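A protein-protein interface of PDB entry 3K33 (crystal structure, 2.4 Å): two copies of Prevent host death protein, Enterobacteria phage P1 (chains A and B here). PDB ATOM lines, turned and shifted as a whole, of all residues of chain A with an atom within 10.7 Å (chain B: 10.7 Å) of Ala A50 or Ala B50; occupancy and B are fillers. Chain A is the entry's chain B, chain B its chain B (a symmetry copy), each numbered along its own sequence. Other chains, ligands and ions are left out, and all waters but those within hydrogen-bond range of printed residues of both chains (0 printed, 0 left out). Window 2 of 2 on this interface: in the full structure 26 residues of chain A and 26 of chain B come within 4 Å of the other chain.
Tyr B47 touches Phe A44. Phe B44 touches Tyr A47. Tyr B47 touches Tyr A47 (O to O, 3.5 Å). Lys B48 touches Tyr A47 (CG to CE2, 3.5 Å). Tyr A47 touches Ala B51. Tyr B47 touches Lys A48. Ala B50 touches Ala A50 (O to CB, 3.999 Å). Ala A50 touches Ala B51. Tyr B47 touches Ala A51 (CD1 to CB, 3.3 Å). CA of Ala A51 touches CB of Ala B50, at 3.6 Å.
Of the printed residues of chain B, Phe A44 touches Tyr B47 (3.8 Å). Of the printed residues of chain B, Lys A48 touches Tyr B47. No residue of chain B comes within 4 Å of Ala A54. Of the printed residues of chain A, Phe B44 touches Tyr A47. No residue of chain A comes within 4 Å of Ala B46. Printed residues of chain A within 4 Å of Tyr B47: Phe A44 (3.8 Å), Tyr A47 (3.5 Å), Lys A48 (3.5 Å) and Ala A51 (3.3 Å). Of the printed residues of chain A, Lys B48 touches Tyr A47 (3.5 Å). No residue of chain A comes within 4 Å of Lys B49. Of the printed residues of chain A, Ala B50 touches Ala A50 (3.999 Å) and Ala A51 (3.6 Å). Of the printed residues of chain A, Ala B51 touches Tyr A47 (3.3 Å) and Ala A50 (3.6 Å). No residue of chain A comes within 4 Å of Asp B53. The nearest printed residue of chain B that does not touch Ala A50 is Ala B54 (4.4 Å). The nearest printed residue of chain A that does not touch Ala B50 is Ala A54 (4.4 Å). The nearest printed residue of chain A that does not touch Tyr B47 is Glu A55 (4.6 Å).
Of the 17 printed residues of chain A, 5 touch a printed residue of chain B. Printed residues of chain A that touch a printed residue of chain B: Phe A44, Tyr A47, Lys A48, Ala A50 and Ala A51. Along chain A the printed residues that touch a printed residue of chain B span positions 44 to 51. Among the printed residues, 10 pairs touch across the chains. Among the printed residues, no Asp or Glu carboxylate lies within 4 Å of a Lys or Arg side-chain nitrogen of the other chain.
Phe A44 touches Tyr B47, and with the chains exchanged Tyr A47 touches Phe B44. Tyr A47 touches its own counterpart, Tyr B47. Tyr A47 touches Lys B48, and with the chains exchanged Lys A48 touches Tyr B47. Ala B50 touches its own counterpart, Ala A50. 17 positions are printed for both chains.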
ATOM      1  N   ALA A  42     -16.436  -9.549  -3.443  1.00  0.00           N
ATOM      2  CA  ALA A  42     -15.672 -10.418  -4.354  1.00  0.00           C
ATOM      3  C   ALA A  42     -14.868 -11.499  -3.620  1.00  0.00           C
ATOM      4  O   ALA A  42     -14.902 -12.673  -3.995  1.00  0.00           O
ATOM      5  CB  ALA A  42     -14.748  -9.587  -5.243  1.00  0.00           C
ATOM      6  N   THR A  43     -14.148 -11.095  -2.577  1.00  0.00           N
ATOM      7  CA  THR A  43     -13.366 -12.024  -1.775  1.00  0.00           C
ATOM      8  C   THR A  43     -14.282 -13.003  -1.054  1.00  0.00           C
ATOM      9  O   THR A  43     -14.020 -14.197  -1.031  1.00  0.00           O
ATOM     10  CB  THR A  43     -12.527 -11.267  -0.748  1.00  0.00           C
ATOM     11  OG1 THR A  43     -11.568 -10.472  -1.440  1.00  0.00           O
ATOM     12  CG2 THR A  43     -11.810 -12.225   0.211  1.00  0.00           C
ATOM     13  N   PHE A  44     -15.355 -12.492  -0.467  1.00  0.00           N
ATOM     14  CA  PHE A  44     -16.322 -13.342   0.233  1.00  0.00           C
ATOM     15  C   PHE A  44     -16.902 -14.396  -0.697  1.00  0.00           C
ATOM     16  O   PHE A  44     -16.900 -15.582  -0.381  1.00  0.00           O
ATOM     17  CB  PHE A  44     -17.468 -12.515   0.813  1.00  0.00           C
ATOM     18  CG  PHE A  44     -18.481 -13.342   1.531  1.00  0.00           C
ATOM     19  CD1 PHE A  44     -18.195 -13.863   2.785  1.00  0.00           C
ATOM     20  CD2 PHE A  44     -19.699 -13.658   0.931  1.00  0.00           C
ATOM     21  CE1 PHE A  44     -19.115 -14.678   3.439  1.00  0.00           C
ATOM     22  CE2 PHE A  44     -20.616 -14.460   1.583  1.00  0.00           C
ATOM     23  CZ  PHE A  44     -20.320 -14.977   2.828  1.00  0.00           C
ATOM     24  N   GLU A  45     -17.410 -13.966  -1.847  1.00  0.00           N
ATOM     25  CA  GLU A  45     -17.974 -14.910  -2.803  1.00  0.00           C
ATOM     26  C   GLU A  45     -16.987 -16.019  -3.170  1.00  0.00           C
ATOM     27  O   GLU A  45     -17.370 -17.183  -3.260  1.00  0.00           O
ATOM     28  CB  GLU A  45     -18.457 -14.187  -4.068  1.00  0.00           C
ATOM     29  CG  GLU A  45     -19.656 -13.246  -3.877  1.00  0.00           C
ATOM     30  CD  GLU A  45     -20.812 -13.836  -3.056  1.00  0.00           C
ATOM     31  OE1 GLU A  45     -21.054 -15.070  -3.094  1.00  0.00           O
ATOM     32  OE2 GLU A  45     -21.499 -13.042  -2.377  1.00  0.00           O
ATOM     33  N   ALA A  46     -15.720 -15.663  -3.371  1.00  0.00           N
ATOM     34  CA  ALA A  46     -14.691 -16.641  -3.729  1.00  0.00           C
ATOM     35  C   ALA A  46     -14.386 -17.599  -2.579  1.00  0.00           C
ATOM     36  O   ALA A  46     -14.066 -18.759  -2.808  1.00  0.00           O
ATOM     37  CB  ALA A  46     -13.410 -15.926  -4.179  1.00  0.00           C
ATOM     38  N   TYR A  47     -14.469 -17.110  -1.343  1.00  0.00           N
ATOM     39  CA  TYR A  47     -14.216 -17.956  -0.177  1.00  0.00           C
ATOM     40  C   TYR A  47     -15.383 -18.916   0.032  1.00  0.00           C
ATOM     41  O   TYR A  47     -15.197 -20.105   0.303  1.00  0.00           O
ATOM     42  CB  TYR A  47     -13.998 -17.090   1.073  1.00  0.00           C
ATOM     43  CG  TYR A  47     -12.654 -16.411   1.119  1.00  0.00           C
ATOM     44  CD1 TYR A  47     -11.762 -16.515   0.054  1.00  0.00           C
ATOM     45  CD2 TYR A  47     -12.271 -15.666   2.224  1.00  0.00           C
ATOM     46  CE1 TYR A  47     -10.504 -15.928   0.105  1.00  0.00           C
ATOM     47  CE2 TYR A  47     -11.019 -15.071   2.284  1.00  0.00           C
ATOM     48  CZ  TYR A  47     -10.140 -15.206   1.224  1.00  0.00           C
ATOM     49  OH  TYR A  47      -8.893 -14.624   1.277  1.00  0.00           O
ATOM     50  N   LYS A  48     -16.592 -18.386  -0.100  1.00  0.00           N
ATOM     51  CA  LYS A  48     -17.803 -19.178   0.051  1.00  0.00           C
ATOM     52  C   LYS A  48     -17.883 -20.268  -1.018  1.00  0.00           C
ATOM     53  O   LYS A  48     -18.248 -21.413  -0.736  1.00  0.00           O
ATOM     54  CB  LYS A  48     -19.025 -18.265  -0.022  1.00  0.00           C
ATOM     55  CG  LYS A  48     -20.336 -18.994   0.268  1.00  0.00           C
ATOM     56  CD  LYS A  48     -21.512 -18.044   0.266  1.00  0.00           C
ATOM     57  CE  LYS A  48     -22.789 -18.783   0.659  1.00  0.00           C
ATOM     58  NZ  LYS A  48     -23.960 -17.857   0.673  1.00  0.00           N
ATOM     59  N   LYS A  49     -17.528 -19.929  -2.247  1.00  0.00           N
ATOM     60  CA  LYS A  49     -17.502 -20.928  -3.315  1.00  0.00           C
ATOM     61  C   LYS A  49     -16.575 -22.108  -2.974  1.00  0.00           C
ATOM     62  O   LYS A  49     -16.921 -23.272  -3.197  1.00  0.00           O
ATOM     63  CB  LYS A  49     -17.040 -20.294  -4.617  1.00  0.00           C
ATOM     64  CG  LYS A  49     -17.009 -21.298  -5.743  1.00  0.00           C
ATOM     65  CD  LYS A  49     -16.398 -20.737  -6.984  1.00  0.00           C
ATOM     66  CE  LYS A  49     -16.358 -21.814  -8.052  1.00  0.00           C
ATOM     67  NZ  LYS A  49     -15.677 -23.030  -7.559  1.00  0.00           N
ATOM     68  N   ALA A  50     -15.394 -21.799  -2.448  1.00  0.00           N
ATOM     69  CA  ALA A  50     -14.419 -22.822  -2.077  1.00  0.00           C
ATOM     70  C   ALA A  50     -14.909 -23.643  -0.873  1.00  0.00           C
ATOM     71  O   ALA A  50     -14.670 -24.851  -0.793  1.00  0.00           O
ATOM     72  CB  ALA A  50     -13.076 -22.161  -1.757  1.00  0.00           C
ATOM     73  N   ALA A  51     -15.603 -22.985   0.052  1.00  0.00           N
ATOM     74  CA  ALA A  51     -16.162 -23.652   1.230  1.00  0.00           C
ATOM     75  C   ALA A  51     -17.253 -24.619   0.816  1.00  0.00           C
ATOM     76  O   ALA A  51     -17.345 -25.719   1.345  1.00  0.00           O
ATOM     77  CB  ALA A  51     -16.720 -22.628   2.217  1.00  0.00           C
ATOM     78  N   LEU A  52     -18.077 -24.205  -0.138  1.00  0.00           N
ATOM     79  CA  LEU A  52     -19.128 -25.061  -0.674  1.00  0.00           C
ATOM     80  C   LEU A  52     -18.574 -26.204  -1.523  1.00  0.00           C
ATOM     81  O   LEU A  52     -19.083 -27.329  -1.464  1.00  0.00           O
ATOM     82  CB  LEU A  52     -20.130 -24.227  -1.480  1.00  0.00           C
ATOM     83  CG  LEU A  52     -21.133 -23.463  -0.625  1.00  0.00           C
ATOM     84  CD1 LEU A  52     -21.880 -22.399  -1.437  1.00  0.00           C
ATOM     85  CD2 LEU A  52     -22.091 -24.463  -0.019  1.00  0.00           C
ATOM     86  N   ASP A  53     -17.550 -25.930  -2.329  1.00  0.00           N
ATOM     87  CA  ASP A  53     -16.892 -27.023  -3.059  1.00  0.00           C
ATOM     88  C   ASP A  53     -16.379 -28.059  -2.068  1.00  0.00           C
ATOM     89  O   ASP A  53     -16.449 -29.255  -2.326  1.00  0.00           O
ATOM     90  CB  ASP A  53     -15.705 -26.527  -3.894  1.00  0.00           C
ATOM     91  CG  ASP A  53     -16.123 -25.611  -5.023  1.00  0.00           C
ATOM     92  OD1 ASP A  53     -17.327 -25.564  -5.352  1.00  0.00           O
ATOM     93  OD2 ASP A  53     -15.236 -24.936  -5.588  1.00  0.00           O
ATOM     94  N   ALA A  54     -15.851 -27.585  -0.935  1.00  0.00           N
ATOM     95  CA  ALA A  54     -15.271 -28.462   0.074  1.00  0.00           C
ATOM     96  C   ALA A  54     -16.367 -29.262   0.769  1.00  0.00           C
ATOM     97  O   ALA A  54     -16.243 -30.467   0.938  1.00  0.00           O
ATOM     98  CB  ALA A  54     -14.465 -27.649   1.093  1.00  0.00           C
ATOM     99  N   GLU A  55     -17.436 -28.579   1.171  1.00  0.00           N
ATOM    100  CA  GLU A  55     -18.550 -29.234   1.838  1.00  0.00           C
ATOM    101  C   GLU A  55     -19.088 -30.323   0.927  1.00  0.00           C
ATOM    102  O   GLU A  55     -19.249 -31.458   1.344  1.00  0.00           O
ATOM    103  CB  GLU A  55     -19.669 -28.235   2.134  1.00  0.00           C
ATOM    104  CG  GLU A  55     -19.320 -27.169   3.158  1.00  0.00           C
ATOM    105  CD  GLU A  55     -20.488 -26.219   3.422  1.00  0.00           C
ATOM    106  OE1 GLU A  55     -20.255 -25.149   4.017  1.00  0.00           O
ATOM    107  OE2 GLU A  55     -21.637 -26.539   3.038  1.00  0.00           O
ATOM    108  N   PHE A  56     -19.358 -29.962  -0.325  1.00  0.00           N
ATOM    109  CA  PHE A  56     -19.837 -30.917  -1.310  1.00  0.00           C
ATOM    110  C   PHE A  56     -18.942 -32.156  -1.434  1.00  0.00           C
ATOM    111  O   PHE A  56     -19.444 -33.278  -1.431  1.00  0.00           O
ATOM    112  CB  PHE A  56     -19.993 -30.249  -2.675  1.00  0.00           C
ATOM    113  CG  PHE A  56     -20.657 -31.133  -3.698  1.00  0.00           C
ATOM    114  CD1 PHE A  56     -22.038 -31.306  -3.690  1.00  0.00           C
ATOM    115  CD2 PHE A  56     -19.892 -31.816  -4.653  1.00  0.00           C
ATOM    116  CE1 PHE A  56     -22.644 -32.158  -4.610  1.00  0.00           C
ATOM    117  CE2 PHE A  56     -20.482 -32.663  -5.564  1.00  0.00           C
ATOM    118  CZ  PHE A  56     -21.867 -32.842  -5.548  1.00  0.00           C
ATOM    119  N   ALA A  57     -17.629 -31.958  -1.570  1.00  0.00           N
ATOM    120  CA  ALA A  57     -16.681 -33.083  -1.629  1.00  0.00           C
ATOM    121  C   ALA A  57     -16.781 -33.981  -0.392  1.00  0.00           C
ATOM    122  O   ALA A  57     -16.778 -35.203  -0.507  1.00  0.00           O
ATOM    123  CB  ALA A  57     -15.225 -32.571  -1.804  1.00  0.00           C
ATOM    124  N   SER A  58     -16.890 -33.366   0.785  1.00  0.00           N
ATOM    125  CA  SER A  58     -16.965 -34.111   2.036  1.00  0.00           C
ATOM    126  C   SER A  58     -18.152 -35.077   2.049  1.00  0.00           C
ATOM    127  O   SER A  58     -18.097 -36.125   2.700  1.00  0.00           O
ATOM    128  CB  SER A  58     -17.039 -33.148   3.233  1.00  0.00           C
ATOM    129  OG  SER A  58     -18.351 -32.596   3.378  1.00  0.00           O
ATOM    130  N   ALA B  42     -16.855 -16.259  12.621  1.00  0.00           N
ATOM    131  CA  ALA B  42     -16.774 -17.729  12.578  1.00  0.00           C
ATOM    132  C   ALA B  42     -16.982 -18.300  11.170  1.00  0.00           C
ATOM    133  O   ALA B  42     -16.216 -19.153  10.717  1.00  0.00           O
ATOM    134  CB  ALA B  42     -17.774 -18.353  13.553  1.00  0.00           C
ATOM    135  N   THR B  43     -18.019 -17.826  10.485  1.00  0.00           N
ATOM    136  CA  THR B  43     -18.310 -18.260   9.127  1.00  0.00           C
ATOM    137  C   THR B  43     -17.196 -17.826   8.183  1.00  0.00           C
ATOM    138  O   THR B  43     -16.745 -18.605   7.355  1.00  0.00           O
ATOM    139  CB  THR B  43     -19.635 -17.670   8.650  1.00  0.00           C
ATOM    140  OG1 THR B  43     -20.686 -18.208   9.446  1.00  0.00           O
ATOM    141  CG2 THR B  43     -19.892 -17.985   7.170  1.00  0.00           C
ATOM    142  N   PHE B  44     -16.756 -16.583   8.313  1.00  0.00           N
ATOM    143  CA  PHE B  44     -15.671 -16.064   7.477  1.00  0.00           C
ATOM    144  C   PHE B  44     -14.408 -16.897   7.637  1.00  0.00           C
ATOM    145  O   PHE B  44     -13.822 -17.343   6.655  1.00  0.00           O
ATOM    146  CB  PHE B  44     -15.347 -14.613   7.828  1.00  0.00           C
ATOM    147  CG  PHE B  44     -14.240 -14.045   7.003  1.00  0.00           C
ATOM    148  CD1 PHE B  44     -14.464 -13.697   5.679  1.00  0.00           C
ATOM    149  CD2 PHE B  44     -12.955 -13.915   7.527  1.00  0.00           C
ATOM    150  CE1 PHE B  44     -13.424 -13.215   4.889  1.00  0.00           C
ATOM    151  CE2 PHE B  44     -11.924 -13.429   6.747  1.00  0.00           C
ATOM    152  CZ  PHE B  44     -12.155 -13.091   5.428  1.00  0.00           C
ATOM    153  N   GLU B  45     -13.981 -17.105   8.877  1.00  0.00           N
ATOM    154  CA  GLU B  45     -12.788 -17.905   9.122  1.00  0.00           C
ATOM    155  C   GLU B  45     -12.874 -19.287   8.472  1.00  0.00           C
ATOM    156  O   GLU B  45     -11.900 -19.761   7.893  1.00  0.00           O
ATOM    157  CB  GLU B  45     -12.516 -18.040  10.626  1.00  0.00           C
ATOM    158  CG  GLU B  45     -12.126 -16.742  11.349  1.00  0.00           C
ATOM    159  CD  GLU B  45     -11.061 -15.902  10.631  1.00  0.00           C
ATOM    160  OE1 GLU B  45     -10.171 -16.461   9.938  1.00  0.00           O
ATOM    161  OE2 GLU B  45     -11.108 -14.662  10.783  1.00  0.00           O
ATOM    162  N   ALA B  46     -14.039 -19.926   8.556  1.00  0.00           N
ATOM    163  CA  ALA B  46     -14.236 -21.254   7.974  1.00  0.00           C
ATOM    164  C   ALA B  46     -14.208 -21.220   6.447  1.00  0.00           C
ATOM    165  O   ALA B  46     -13.765 -22.171   5.814  1.00  0.00           O
ATOM    166  CB  ALA B  46     -15.554 -21.864   8.466  1.00  0.00           C
ATOM    167  N   TYR B  47     -14.694 -20.130   5.855  1.00  0.00           N
ATOM    168  CA  TYR B  47     -14.690 -19.996   4.398  1.00  0.00           C
ATOM    169  C   TYR B  47     -13.271 -19.735   3.904  1.00  0.00           C
ATOM    170  O   TYR B  47     -12.819 -20.312   2.912  1.00  0.00           O
ATOM    171  CB  TYR B  47     -15.630 -18.861   3.965  1.00  0.00           C
ATOM    172  CG  TYR B  47     -17.093 -19.211   4.053  1.00  0.00           C
ATOM    173  CD1 TYR B  47     -17.506 -20.435   4.577  1.00  0.00           C
ATOM    174  CD2 TYR B  47     -18.065 -18.326   3.615  1.00  0.00           C
ATOM    175  CE1 TYR B  47     -18.849 -20.786   4.622  1.00  0.00           C
ATOM    176  CE2 TYR B  47     -19.410 -18.663   3.659  1.00  0.00           C
ATOM    177  CZ  TYR B  47     -19.796 -19.893   4.162  1.00  0.00           C
ATOM    178  OH  TYR B  47     -21.129 -20.239   4.206  1.00  0.00           O
ATOM    179  N   LYS B  48     -12.571 -18.857   4.611  1.00  0.00           N
ATOM    180  CA  LYS B  48     -11.196 -18.516   4.275  1.00  0.00           C
ATOM    181  C   LYS B  48     -10.282 -19.737   4.401  1.00  0.00           C
ATOM    182  O   LYS B  48      -9.417 -19.976   3.554  1.00  0.00           O
ATOM    183  CB  LYS B  48     -10.712 -17.388   5.182  1.00  0.00           C
ATOM    184  CG  LYS B  48      -9.324 -16.870   4.806  1.00  0.00           C
ATOM    185  CD  LYS B  48      -8.913 -15.702   5.672  1.00  0.00           C
ATOM    186  CE  LYS B  48      -7.571 -15.144   5.206  1.00  0.00           C
ATOM    187  NZ  LYS B  48      -7.154 -13.981   6.045  1.00  0.00           N
ATOM    188  N   LYS B  49     -10.475 -20.523   5.448  1.00  0.00           N
ATOM    189  CA  LYS B  49      -9.697 -21.751   5.606  1.00  0.00           C
ATOM    190  C   LYS B  49      -9.858 -22.692   4.400  1.00  0.00           C
ATOM    191  O   LYS B  49      -8.883 -23.272   3.911  1.00  0.00           O
ATOM    192  CB  LYS B  49     -10.123 -22.485   6.868  1.00  0.00           C
ATOM    193  CG  LYS B  49      -9.333 -23.756   7.065  1.00  0.00           C
ATOM    194  CD  LYS B  49      -9.851 -24.573   8.202  1.00  0.00           C
ATOM    195  CE  LYS B  49      -9.041 -25.850   8.307  1.00  0.00           C
ATOM    196  NZ  LYS B  49      -9.020 -26.579   7.022  1.00  0.00           N
ATOM    197  N   ALA B  50     -11.094 -22.852   3.935  1.00  0.00           N
ATOM    198  CA  ALA B  50     -11.387 -23.715   2.793  1.00  0.00           C
ATOM    199  C   ALA B  50     -10.812 -23.130   1.494  1.00  0.00           C
ATOM    200  O   ALA B  50     -10.349 -23.868   0.619  1.00  0.00           O
ATOM    201  CB  ALA B  50     -12.900 -23.903   2.666  1.00  0.00           C
ATOM    202  N   ALA B  51     -10.835 -21.804   1.378  1.00  0.00           N
ATOM    203  CA  ALA B  51     -10.284 -21.112   0.210  1.00  0.00           C
ATOM    204  C   ALA B  51      -8.779 -21.291   0.157  1.00  0.00           C
ATOM    205  O   ALA B  51      -8.214 -21.502  -0.907  1.00  0.00           O
ATOM    206  CB  ALA B  51     -10.633 -19.626   0.248  1.00  0.00           C
ATOM    207  N   LEU B  52      -8.135 -21.207   1.314  1.00  0.00           N
ATOM    208  CA  LEU B  52      -6.697 -21.423   1.412  1.00  0.00           C
ATOM    209  C   LEU B  52      -6.311 -22.886   1.198  1.00  0.00           C
ATOM    210  O   LEU B  52      -5.290 -23.175   0.561  1.00  0.00           O
ATOM    211  CB  LEU B  52      -6.177 -20.922   2.764  1.00  0.00           C
ATOM    212  CG  LEU B  52      -5.997 -19.410   2.837  1.00  0.00           C
ATOM    213  CD1 LEU B  52      -5.807 -18.928   4.280  1.00  0.00           C
ATOM    214  CD2 LEU B  52      -4.812 -19.037   1.976  1.00  0.00           C
ATOM    215  N   ASP B  53      -7.098 -23.815   1.737  1.00  0.00           N
ATOM    216  CA  ASP B  53      -6.849 -25.233   1.440  1.00  0.00           C
ATOM    217  C   ASP B  53      -6.908 -25.456  -0.065  1.00  0.00           C
ATOM    218  O   ASP B  53      -6.127 -26.229  -0.609  1.00  0.00           O
ATOM    219  CB  ASP B  53      -7.883 -26.151   2.103  1.00  0.00           C
ATOM    220  CG  ASP B  53      -7.803 -26.133   3.614  1.00  0.00           C
ATOM    221  OD1 ASP B  53      -6.793 -25.644   4.162  1.00  0.00           O
ATOM    222  OD2 ASP B  53      -8.759 -26.617   4.257  1.00  0.00           O
ATOM    223  N   ALA B  54      -7.851 -24.780  -0.728  1.00  0.00           N
ATOM    224  CA  ALA B  54      -8.055 -24.944  -2.162  1.00  0.00           C
ATOM    225  C   ALA B  54      -6.892 -24.330  -2.933  1.00  0.00           C
ATOM    226  O   ALA B  54      -6.358 -24.945  -3.845  1.00  0.00           O
ATOM    227  CB  ALA B  54      -9.383 -24.311  -2.590  1.00  0.00           C
ATOM    228  N   GLU B  55      -6.510 -23.111  -2.558  1.00  0.00           N
ATOM    229  CA  GLU B  55      -5.406 -22.425  -3.212  1.00  0.00           C
ATOM    230  C   GLU B  55      -4.163 -23.290  -3.099  1.00  0.00           C
ATOM    231  O   GLU B  55      -3.497 -23.552  -4.087  1.00  0.00           O
ATOM    232  CB  GLU B  55      -5.136 -21.076  -2.550  1.00  0.00           C
ATOM    233  CG  GLU B  55      -6.242 -20.047  -2.719  1.00  0.00           C
ATOM    234  CD  GLU B  55      -5.897 -18.715  -2.051  1.00  0.00           C
ATOM    235  OE1 GLU B  55      -6.815 -17.891  -1.873  1.00  0.00           O
ATOM    236  OE2 GLU B  55      -4.713 -18.491  -1.706  1.00  0.00           O
ATOM    237  N   PHE B  56      -3.864 -23.732  -1.880  1.00  0.00           N
ATOM    238  CA  PHE B  56      -2.725 -24.603  -1.641  1.00  0.00           C
ATOM    239  C   PHE B  56      -2.722 -25.852  -2.532  1.00  0.00           C
ATOM    240  O   PHE B  56      -1.698 -26.177  -3.126  1.00  0.00           O
ATOM    241  CB  PHE B  56      -2.662 -25.014  -0.170  1.00  0.00           C
ATOM    242  CG  PHE B  56      -1.407 -25.767   0.184  1.00  0.00           C
ATOM    243  CD1 PHE B  56      -0.209 -25.086   0.383  1.00  0.00           C
ATOM    244  CD2 PHE B  56      -1.422 -27.163   0.289  1.00  0.00           C
ATOM    245  CE1 PHE B  56       0.958 -25.790   0.668  1.00  0.00           C
ATOM    246  CE2 PHE B  56      -0.271 -27.868   0.567  1.00  0.00           C
ATOM    247  CZ  PHE B  56       0.932 -27.183   0.759  1.00  0.00           C
ATOM    248  N   ALA B  57      -3.851 -26.560  -2.605  1.00  0.00           N
ATOM    249  CA  ALA B  57      -3.968 -27.735  -3.485  1.00  0.00           C
ATOM    250  C   ALA B  57      -3.670 -27.387  -4.946  1.00  0.00           C
ATOM    251  O   ALA B  57      -2.965 -28.124  -5.631  1.00  0.00           O
ATOM    252  CB  ALA B  57      -5.377 -28.378  -3.364  1.00  0.00           C
ATOM    253  N   SER B  58      -4.192 -26.252  -5.409  1.00  0.00           N
ATOM    254  CA  SER B  58      -4.002 -25.827  -6.790  1.00  0.00           C
ATOM    255  C   SER B  58      -2.519 -25.681  -7.137  1.00  0.00           C
ATOM    256  O   SER B  58      -2.127 -25.870  -8.294  1.00  0.00           O
ATOM    257  CB  SER B  58      -4.750 -24.510  -7.057  1.00  0.00           C
ATOM    258  OG  SER B  58      -4.043 -23.389  -6.519  1.00  0.00           O
